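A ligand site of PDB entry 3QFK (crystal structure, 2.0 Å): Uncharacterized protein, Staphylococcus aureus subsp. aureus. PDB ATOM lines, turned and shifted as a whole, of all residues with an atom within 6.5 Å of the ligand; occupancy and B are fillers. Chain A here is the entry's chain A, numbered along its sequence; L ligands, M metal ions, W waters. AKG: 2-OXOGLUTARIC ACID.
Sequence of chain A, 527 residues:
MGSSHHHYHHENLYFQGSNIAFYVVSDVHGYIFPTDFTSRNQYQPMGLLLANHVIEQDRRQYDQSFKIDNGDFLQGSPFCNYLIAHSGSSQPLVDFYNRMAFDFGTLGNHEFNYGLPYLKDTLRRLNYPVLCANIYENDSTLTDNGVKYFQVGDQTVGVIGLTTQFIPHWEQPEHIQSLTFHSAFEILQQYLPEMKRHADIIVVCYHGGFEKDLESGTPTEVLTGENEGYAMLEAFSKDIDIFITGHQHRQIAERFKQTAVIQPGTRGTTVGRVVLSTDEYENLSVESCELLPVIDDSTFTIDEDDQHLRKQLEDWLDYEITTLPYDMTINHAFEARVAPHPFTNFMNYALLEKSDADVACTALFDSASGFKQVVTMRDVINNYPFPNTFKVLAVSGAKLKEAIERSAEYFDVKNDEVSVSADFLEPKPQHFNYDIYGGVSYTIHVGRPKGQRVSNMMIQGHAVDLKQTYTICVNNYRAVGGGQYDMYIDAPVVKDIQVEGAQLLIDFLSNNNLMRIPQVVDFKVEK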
ATOM      1  N   HIS A  29       9.022 -18.094  17.405  1.00  0.00           N
ATOM      2  CA  HIS A  29       7.627 -17.727  17.227  1.00  0.00           C
ATOM      3  C   HIS A  29       6.619 -18.304  18.247  1.00  0.00           C
ATOM      4  O   HIS A  29       5.464 -18.537  17.919  1.00  0.00           O
ATOM      5  CB  HIS A  29       7.170 -18.052  15.779  1.00  0.00           C
ATOM      6  CG  HIS A  29       7.577 -17.016  14.762  1.00  0.00           C
ATOM      7  ND1 HIS A  29       7.037 -15.742  14.765  1.00  0.00           N
ATOM      8  CD2 HIS A  29       8.442 -17.058  13.721  1.00  0.00           C
ATOM      9  CE1 HIS A  29       7.568 -15.042  13.774  1.00  0.00           C
ATOM     10  NE2 HIS A  29       8.431 -15.824  13.128  1.00  0.00           N
ATOM     11  N   ASP A  72      11.783 -12.537  16.786  1.00  0.00           N
ATOM     12  CA  ASP A  72      10.515 -13.179  16.436  1.00  0.00           C
ATOM     13  C   ASP A  72      10.202 -14.295  17.437  1.00  0.00           C
ATOM     14  O   ASP A  72       9.926 -15.426  17.046  1.00  0.00           O
ATOM     15  CB  ASP A  72      10.498 -13.649  14.980  1.00  0.00           C
ATOM     16  CG  ASP A  72      10.095 -12.552  14.034  1.00  0.00           C
ATOM     17  OD1 ASP A  72       9.966 -11.403  14.480  1.00  0.00           O
ATOM     18  OD2 ASP A  72       9.850 -12.830  12.862  1.00  0.00           O
ATOM     19  N   ASN A 109      10.792  -8.285  13.881  1.00  0.00           N
ATOM     20  CA  ASN A 109       9.647  -7.432  13.560  1.00  0.00           C
ATOM     21  C   ASN A 109       8.367  -7.808  14.336  1.00  0.00           C
ATOM     22  O   ASN A 109       7.570  -6.933  14.688  1.00  0.00           O
ATOM     23  CB  ASN A 109       9.322  -7.399  12.050  1.00  0.00           C
ATOM     24  CG  ASN A 109       9.192  -8.789  11.449  1.00  0.00           C
ATOM     25  OD1 ASN A 109      10.129  -9.604  11.535  1.00  0.00           O
ATOM     26  ND2 ASN A 109       8.049  -9.068  10.818  1.00  0.00           N
ATOM     27  N   HIS A 110       8.178  -9.094  14.604  1.00  0.00           N
ATOM     28  CA  HIS A 110       6.985  -9.534  15.311  1.00  0.00           C
ATOM     29  C   HIS A 110       6.909  -9.147  16.797  1.00  0.00           C
ATOM     30  O   HIS A 110       5.817  -9.199  17.366  1.00  0.00           O
ATOM     31  CB  HIS A 110       6.671 -11.011  15.059  1.00  0.00           C
ATOM     32  CG  HIS A 110       6.249 -11.281  13.647  1.00  0.00           C
ATOM     33  ND1 HIS A 110       4.984 -10.984  13.183  1.00  0.00           N
ATOM     34  CD2 HIS A 110       6.938 -11.772  12.584  1.00  0.00           C
ATOM     35  CE1 HIS A 110       4.899 -11.301  11.902  1.00  0.00           C
ATOM     36  NE2 HIS A 110       6.073 -11.772  11.504  1.00  0.00           N
ATOM     37  N   ASN A 113       4.062  -6.516  17.290  1.00  0.00           N
ATOM     38  CA  ASN A 113       2.686  -6.853  16.925  1.00  0.00           C
ATOM     39  C   ASN A 113       1.612  -6.527  17.976  1.00  0.00           C
ATOM     40  O   ASN A 113       0.469  -6.365  17.621  1.00  0.00           O
ATOM     41  CB  ASN A 113       2.551  -8.351  16.571  1.00  0.00           C
ATOM     42  CG  ASN A 113       3.072  -8.712  15.169  1.00  0.00           C
ATOM     43  OD1 ASN A 113       3.050  -9.876  14.786  1.00  0.00           O
ATOM     44  ND2 ASN A 113       3.492  -7.711  14.379  1.00  0.00           N
ATOM     45  N   TRP A 170       4.963  -2.677   7.795  1.00  0.00           N
ATOM     46  CA  TRP A 170       4.175  -3.798   8.260  1.00  0.00           C
ATOM     47  C   TRP A 170       3.275  -3.573   9.468  1.00  0.00           C
ATOM     48  O   TRP A 170       2.173  -4.114   9.545  1.00  0.00           O
ATOM     49  CB  TRP A 170       5.138  -4.949   8.647  1.00  0.00           C
ATOM     50  CG  TRP A 170       6.083  -5.356   7.524  1.00  0.00           C
ATOM     51  CD1 TRP A 170       5.784  -5.443   6.183  1.00  0.00           C
ATOM     52  CD2 TRP A 170       7.409  -5.869   7.668  1.00  0.00           C
ATOM     53  NE1 TRP A 170       6.880  -5.888   5.478  1.00  0.00           N
ATOM     54  CE2 TRP A 170       7.886  -6.170   6.366  1.00  0.00           C
ATOM     55  CE3 TRP A 170       8.263  -6.062   8.766  1.00  0.00           C
ATOM     56  CZ2 TRP A 170       9.159  -6.681   6.144  1.00  0.00           C
ATOM     57  CZ3 TRP A 170       9.538  -6.542   8.537  1.00  0.00           C
ATOM     58  CH2 TRP A 170       9.975  -6.843   7.235  1.00  0.00           C
ATOM     59  N   HIS A 247      14.850 -13.951  10.290  1.00  0.00           N
ATOM     60  CA  HIS A 247      13.785 -13.281   9.534  1.00  0.00           C
ATOM     61  C   HIS A 247      13.227 -14.022   8.305  1.00  0.00           C
ATOM     62  O   HIS A 247      12.021 -14.070   8.130  1.00  0.00           O
ATOM     63  CB  HIS A 247      14.241 -11.860   9.121  1.00  0.00           C
ATOM     64  CG  HIS A 247      13.161 -11.059   8.449  1.00  0.00           C
ATOM     65  ND1 HIS A 247      11.993 -10.727   9.092  1.00  0.00           N
ATOM     66  CD2 HIS A 247      13.089 -10.515   7.204  1.00  0.00           C
ATOM     67  CE1 HIS A 247      11.234 -10.022   8.272  1.00  0.00           C
ATOM     68  NE2 HIS A 247      11.876  -9.869   7.124  1.00  0.00           N
ATOM     69  N   HIS A 249      13.591 -17.255   7.668  1.00  0.00           N
ATOM     70  CA  HIS A 249      13.242 -18.636   7.988  1.00  0.00           C
ATOM     71  C   HIS A 249      14.000 -19.656   7.144  1.00  0.00           C
ATOM     72  O   HIS A 249      13.523 -20.775   6.942  1.00  0.00           O
ATOM     73  CB  HIS A 249      11.726 -18.839   7.789  1.00  0.00           C
ATOM     74  CG  HIS A 249      10.878 -18.029   8.712  1.00  0.00           C
ATOM     75  ND1 HIS A 249       9.523 -18.253   8.863  1.00  0.00           N
ATOM     76  CD2 HIS A 249      11.196 -17.067   9.614  1.00  0.00           C
ATOM     77  CE1 HIS A 249       9.034 -17.403   9.756  1.00  0.00           C
ATOM     78  NE2 HIS A 249      10.036 -16.682  10.234  1.00  0.00           N
ATOM     79  N   ALA A 363      -6.029 -13.060   2.086  1.00  0.00           N
ATOM     80  CA  ALA A 363      -5.138 -14.073   1.619  1.00  0.00           C
ATOM     81  C   ALA A 363      -5.622 -15.372   2.205  1.00  0.00           C
ATOM     82  O   ALA A 363      -6.406 -15.381   3.157  1.00  0.00           O
ATOM     83  CB  ALA A 363      -3.699 -13.776   2.058  1.00  0.00           C
ATOM     84  N   PHE A 365      -4.119 -18.169   4.020  1.00  0.00           N
ATOM     85  CA  PHE A 365      -2.853 -18.435   4.653  1.00  0.00           C
ATOM     86  C   PHE A 365      -2.422 -19.903   4.518  1.00  0.00           C
ATOM     87  O   PHE A 365      -3.254 -20.794   4.282  1.00  0.00           O
ATOM     88  CB  PHE A 365      -2.887 -17.964   6.107  1.00  0.00           C
ATOM     89  CG  PHE A 365      -3.299 -16.526   6.244  1.00  0.00           C
ATOM     90  CD1 PHE A 365      -2.510 -15.508   5.716  1.00  0.00           C
ATOM     91  CD2 PHE A 365      -4.465 -16.178   6.921  1.00  0.00           C
ATOM     92  CE1 PHE A 365      -2.874 -14.172   5.854  1.00  0.00           C
ATOM     93  CE2 PHE A 365      -4.851 -14.831   7.065  1.00  0.00           C
ATOM     94  CZ  PHE A 365      -4.050 -13.833   6.527  1.00  0.00           C
ATOM     95  N   TYR A 384      -6.899 -18.050  10.363  1.00  0.00           N
ATOM     96  CA  TYR A 384      -6.467 -16.646  10.461  1.00  0.00           C
ATOM     97  C   TYR A 384      -5.537 -16.521  11.675  1.00  0.00           C
ATOM     98  O   TYR A 384      -5.962 -16.079  12.705  1.00  0.00           O
ATOM     99  CB  TYR A 384      -7.667 -15.672  10.586  1.00  0.00           C
ATOM    100  CG  TYR A 384      -7.294 -14.331   9.998  1.00  0.00           C
ATOM    101  CD1 TYR A 384      -6.374 -13.514  10.611  1.00  0.00           C
ATOM    102  CD2 TYR A 384      -7.806 -13.935   8.761  1.00  0.00           C
ATOM    103  CE1 TYR A 384      -5.956 -12.326  10.028  1.00  0.00           C
ATOM    104  CE2 TYR A 384      -7.408 -12.755   8.172  1.00  0.00           C
ATOM    105  CZ  TYR A 384      -6.493 -11.950   8.803  1.00  0.00           C
ATOM    106  OH  TYR A 384      -6.077 -10.773   8.228  1.00  0.00           O
ATOM    107  N   PHE A 386      -2.959 -14.477  12.407  1.00  0.00           N
ATOM    108  CA  PHE A 386      -2.226 -13.233  12.553  1.00  0.00           C
ATOM    109  C   PHE A 386      -3.116 -12.270  13.294  1.00  0.00           C
ATOM    110  O   PHE A 386      -4.329 -12.297  13.109  1.00  0.00           O
ATOM    111  CB  PHE A 386      -1.834 -12.651  11.191  1.00  0.00           C
ATOM    112  CG  PHE A 386      -0.892 -13.530  10.420  1.00  0.00           C
ATOM    113  CD1 PHE A 386       0.451 -13.613  10.771  1.00  0.00           C
ATOM    114  CD2 PHE A 386      -1.356 -14.289   9.347  1.00  0.00           C
ATOM    115  CE1 PHE A 386       1.328 -14.438  10.062  1.00  0.00           C
ATOM    116  CE2 PHE A 386      -0.484 -15.102   8.618  1.00  0.00           C
ATOM    117  CZ  PHE A 386       0.859 -15.176   8.970  1.00  0.00           C
ATOM    118  N   PRO A 387      -2.532 -11.417  14.148  1.00  0.00           N
ATOM    119  CA  PRO A 387      -3.377 -10.483  14.867  1.00  0.00           C
ATOM    120  C   PRO A 387      -3.661  -9.210  14.053  1.00  0.00           C
ATOM    121  O   PRO A 387      -3.529  -8.131  14.558  1.00  0.00           O
ATOM    122  CB  PRO A 387      -2.568 -10.172  16.143  1.00  0.00           C
ATOM    123  CG  PRO A 387      -1.171 -10.355  15.761  1.00  0.00           C
ATOM    124  CD  PRO A 387      -1.127 -11.308  14.568  1.00  0.00           C
ATOM    125  N   ASN A 388      -4.099  -9.357  12.806  1.00  0.00           N
ATOM    126  CA  ASN A 388      -4.385  -8.204  11.979  1.00  0.00           C
ATOM    127  C   ASN A 388      -5.772  -7.647  12.250  1.00  0.00           C
ATOM    128  O   ASN A 388      -6.706  -8.399  12.491  1.00  0.00           O
ATOM    129  CB  ASN A 388      -4.350  -8.581  10.494  1.00  0.00           C
ATOM    130  CG  ASN A 388      -3.015  -9.179  10.050  1.00  0.00           C
ATOM    131  OD1 ASN A 388      -1.986  -8.879  10.603  1.00  0.00           O
ATOM    132  ND2 ASN A 388      -3.062 -10.039   9.031  1.00  0.00           N
ATOM    133  N   LYS A 428      11.623 -17.580   0.734  1.00  0.00           N
ATOM    134  CA  LYS A 428      10.637 -17.860   1.792  1.00  0.00           C
ATOM    135  C   LYS A 428       9.221 -17.838   1.187  1.00  0.00           C
ATOM    136  O   LYS A 428       8.889 -16.918   0.467  1.00  0.00           O
ATOM    137  CB  LYS A 428      10.713 -16.832   2.930  1.00  0.00           C
ATOM    138  CG  LYS A 428       9.653 -17.063   4.006  1.00  0.00           C
ATOM    139  CD  LYS A 428       9.666 -16.010   5.111  1.00  0.00           C
ATOM    140  CE  LYS A 428       8.526 -16.250   6.092  1.00  0.00           C
ATOM    141  NZ  LYS A 428       8.377 -15.165   7.108  1.00  0.00           N
ATOM    142  N   PHE A 432       0.751 -15.479   1.938  1.00  0.00           N
ATOM    143  CA  PHE A 432       0.037 -14.410   2.612  1.00  0.00           C
ATOM    144  C   PHE A 432       0.007 -13.128   1.770  1.00  0.00           C
ATOM    145  O   PHE A 432      -0.716 -12.189   2.085  1.00  0.00           O
ATOM    146  CB  PHE A 432       0.617 -14.112   4.015  1.00  0.00           C
ATOM    147  CG  PHE A 432       2.100 -13.827   4.028  1.00  0.00           C
ATOM    148  CD1 PHE A 432       2.574 -12.575   3.684  1.00  0.00           C
ATOM    149  CD2 PHE A 432       3.016 -14.796   4.422  1.00  0.00           C
ATOM    150  CE1 PHE A 432       3.932 -12.308   3.694  1.00  0.00           C
ATOM    151  CE2 PHE A 432       4.374 -14.540   4.431  1.00  0.00           C
ATOM    152  CZ  PHE A 432       4.834 -13.295   4.062  1.00  0.00           C
ATOM    153  N   ASN A 433       0.820 -13.076   0.706  1.00  0.00           N
ATOM    154  CA  ASN A 433       0.828 -11.910  -0.181  1.00  0.00           C
ATOM    155  C   ASN A 433      -0.005 -12.059  -1.456  1.00  0.00           C
ATOM    156  O   ASN A 433       0.081 -11.226  -2.338  1.00  0.00           O
ATOM    157  CB  ASN A 433       2.257 -11.420  -0.460  1.00  0.00           C
ATOM    158  CG  ASN A 433       2.849 -10.663   0.717  1.00  0.00           C
ATOM    159  OD1 ASN A 433       2.123  -9.999   1.498  1.00  0.00           O
ATOM    160  ND2 ASN A 433       4.151 -10.744   0.861  1.00  0.00           N
ATOM    161  N   ASN A 475      -6.612  -5.832   5.338  1.00  0.00           N
ATOM    162  CA  ASN A 475      -6.036  -5.971   6.693  1.00  0.00           C
ATOM    163  C   ASN A 475      -5.023  -4.822   6.941  1.00  0.00           C
ATOM    164  O   ASN A 475      -4.575  -4.195   5.982  1.00  0.00           O
ATOM    165  CB  ASN A 475      -5.476  -7.366   6.961  1.00  0.00           C
ATOM    166  CG  ASN A 475      -4.194  -7.655   6.196  1.00  0.00           C
ATOM    167  OD1 ASN A 475      -3.307  -6.830   6.117  1.00  0.00           O
ATOM    168  ND2 ASN A 475      -4.080  -8.876   5.675  1.00  0.00           N
ATOM    169  N   ASN A 476      -4.657  -4.575   8.202  1.00  0.00           N
ATOM    170  CA  ASN A 476      -3.777  -3.454   8.527  1.00  0.00           C
ATOM    171  C   ASN A 476      -2.386  -3.602   7.929  1.00  0.00           C
ATOM    172  O   ASN A 476      -1.750  -2.605   7.598  1.00  0.00           O
ATOM    173  CB  ASN A 476      -3.671  -3.233  10.041  1.00  0.00           C
ATOM    174  CG  ASN A 476      -2.918  -4.346  10.741  1.00  0.00           C
ATOM    175  OD1 ASN A 476      -3.444  -5.450  10.943  1.00  0.00           O
ATOM    176  ND2 ASN A 476      -1.671  -4.060  11.120  1.00  0.00           N
ATOM    177  N   TYR A 477      -1.940  -4.837   7.771  1.00  0.00           N
ATOM    178  CA  TYR A 477      -0.641  -5.102   7.147  1.00  0.00           C
ATOM    179  C   TYR A 477      -0.658  -4.530   5.733  1.00  0.00           C
ATOM    180  O   TYR A 477       0.232  -3.780   5.335  1.00  0.00           O
ATOM    181  CB  TYR A 477      -0.365  -6.613   7.134  1.00  0.00           C
ATOM    182  CG  TYR A 477       0.947  -7.055   6.556  1.00  0.00           C
ATOM    183  CD1 TYR A 477       2.084  -7.147   7.363  1.00  0.00           C
ATOM    184  CD2 TYR A 477       1.040  -7.482   5.246  1.00  0.00           C
ATOM    185  CE1 TYR A 477       3.306  -7.606   6.854  1.00  0.00           C
ATOM    186  CE2 TYR A 477       2.256  -7.939   4.726  1.00  0.00           C
ATOM    187  CZ  TYR A 477       3.383  -7.991   5.534  1.00  0.00           C
ATOM    188  OH  TYR A 477       4.562  -8.461   5.034  1.00  0.00           O
ATOM    189  N   ARG A 478      -1.688  -4.856   4.970  1.00  0.00           N
ATOM    190  CA  ARG A 478      -1.820  -4.287   3.598  1.00  0.00           C
ATOM    191  C   ARG A 478      -1.954  -2.805   3.582  1.00  0.00           C
ATOM    192  O   ARG A 478      -1.433  -2.153   2.665  1.00  0.00           O
ATOM    193  CB  ARG A 478      -3.086  -4.768   2.893  1.00  0.00           C
ATOM    194  CG  ARG A 478      -3.044  -6.096   2.436  1.00  0.00           C
ATOM    195  CD  ARG A 478      -2.186  -6.273   1.160  1.00  0.00           C
ATOM    196  NE  ARG A 478      -2.242  -7.690   0.876  1.00  0.00           N
ATOM    197  CZ  ARG A 478      -1.369  -8.591   1.288  1.00  0.00           C
ATOM    198  NH1 ARG A 478      -0.267  -8.241   1.927  1.00  0.00           N
ATOM    199  NH2 ARG A 478      -1.586  -9.875   1.009  1.00  0.00           N
HETATM  200  C1  AKG L   1       4.646 -12.588   8.159  1.00  0.00           C
HETATM  201  O1  AKG L   1       4.459 -13.818   8.018  1.00  0.00           O
HETATM  202  O2  AKG L   1       5.788 -12.140   8.363  1.00  0.00           O
HETATM  203  C2  AKG L   1       3.521 -11.644   8.103  1.00  0.00           C
HETATM  204  O5  AKG L   1       3.688 -10.529   8.558  1.00  0.00           O
HETATM  205  C3  AKG L   1       2.178 -12.046   7.511  1.00  0.00           C
HETATM  206  C4  AKG L   1       1.453 -10.875   6.834  1.00  0.00           C
HETATM  207  C5  AKG L   1       0.070 -10.654   7.411  1.00  0.00           C
HETATM  208  O3  AKG L   1      -0.928 -10.763   6.680  1.00  0.00           O
HETATM  209  O4  AKG L   1      -0.024 -10.367   8.622  1.00  0.00           O
HETATM  210 ZN    ZN M   1       9.854 -14.789  11.672  1.00  0.00          ZN
HETATM  211 MN    MN M   2      10.997 -11.536  11.189  1.00  0.00          MN
HETATM  212  O   HOH W   1      -2.082 -10.547   4.513  1.00  0.00           O
HETATM  213  O   HOH W   2       8.158 -11.930   9.317  1.00  0.00           O
HETATM  214  O   HOH W   3       6.492  -9.164   7.073  1.00  0.00           O
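The side-chain hydroxyl (OH) of Tyr 384 is in hydrogen-bond range of the side-chain amide nitrogen (ND2) of Asn 388 (3.2 Å).
NE2 of His 110 sits close to ND2 of Asn 109 (3.4 Å).
The side-chain carboxylate (OD1) of Asp 72 sits at hydrogen-bond distance from the backbone NH (N) of His 110 (2.9 Å).
The side-chain amide oxygen (OD1) of Asn 113 is in hydrogen-bond range of a ring nitrogen (ND1) of His 110, 2.7 Å away.
The backbone NH (N) of Tyr 477 lies within hydrogen-bond range of the side-chain amide oxygen (OD1) of Asn 475, at 2.9 Å.
OH of Tyr 477 sits close to NE1 of Trp 170, at 3.5 Å.
The backbone carbonyl oxygen of Phe 432 is in hydrogen-bond range of the guanidinium group of Arg 478 (2.7 Å).
The side-chain amide oxygen of Asn 475 sits at hydrogen-bond distance from the backbone NH of Arg 478.
ND2 of Asn 388 is in hydrogen-bond range of O4 of the ligand (3.1 Å).
A ring nitrogen (NE2) of His 110 is in hydrogen-bond range of an oxygen (O2) of the ligand (3.2 Å).
Water W1 lies within hydrogen-bond range of an oxygen (O3) of the ligand (2.5 Å), the side-chain amide nitrogen (ND2) of Asn 475 (2.9 Å) and the backbone carbonyl oxygen (O) of Phe 432 (3.2 Å).
Water W2 lies within hydrogen-bond range of O2 of the ligand, NE2 of His 110 and ND2 of Asn 109.
Water W3 bridges the side-chain hydroxyl (OH) of Tyr 477 (2.9 Å) and an oxygen (O2) of the ligand (3.3 Å).
CE1 of Phe 386 touches C3 of the ligand (3.6 Å).
Phe 432 touches the ligand.
Asn 475 touches the ligand.
CE1 of Tyr 477 touches O5 of the ligand, 3.4 Å away.
Hydrophobic or aromatic side chains that line the ligand: His 110, Phe 386, Phe 432 and Tyr 477.
Six residues have an atom within 4 Å of the ligand: His 110, Phe 386, Asn 388, Phe 432, Asn 475 and Tyr 477.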
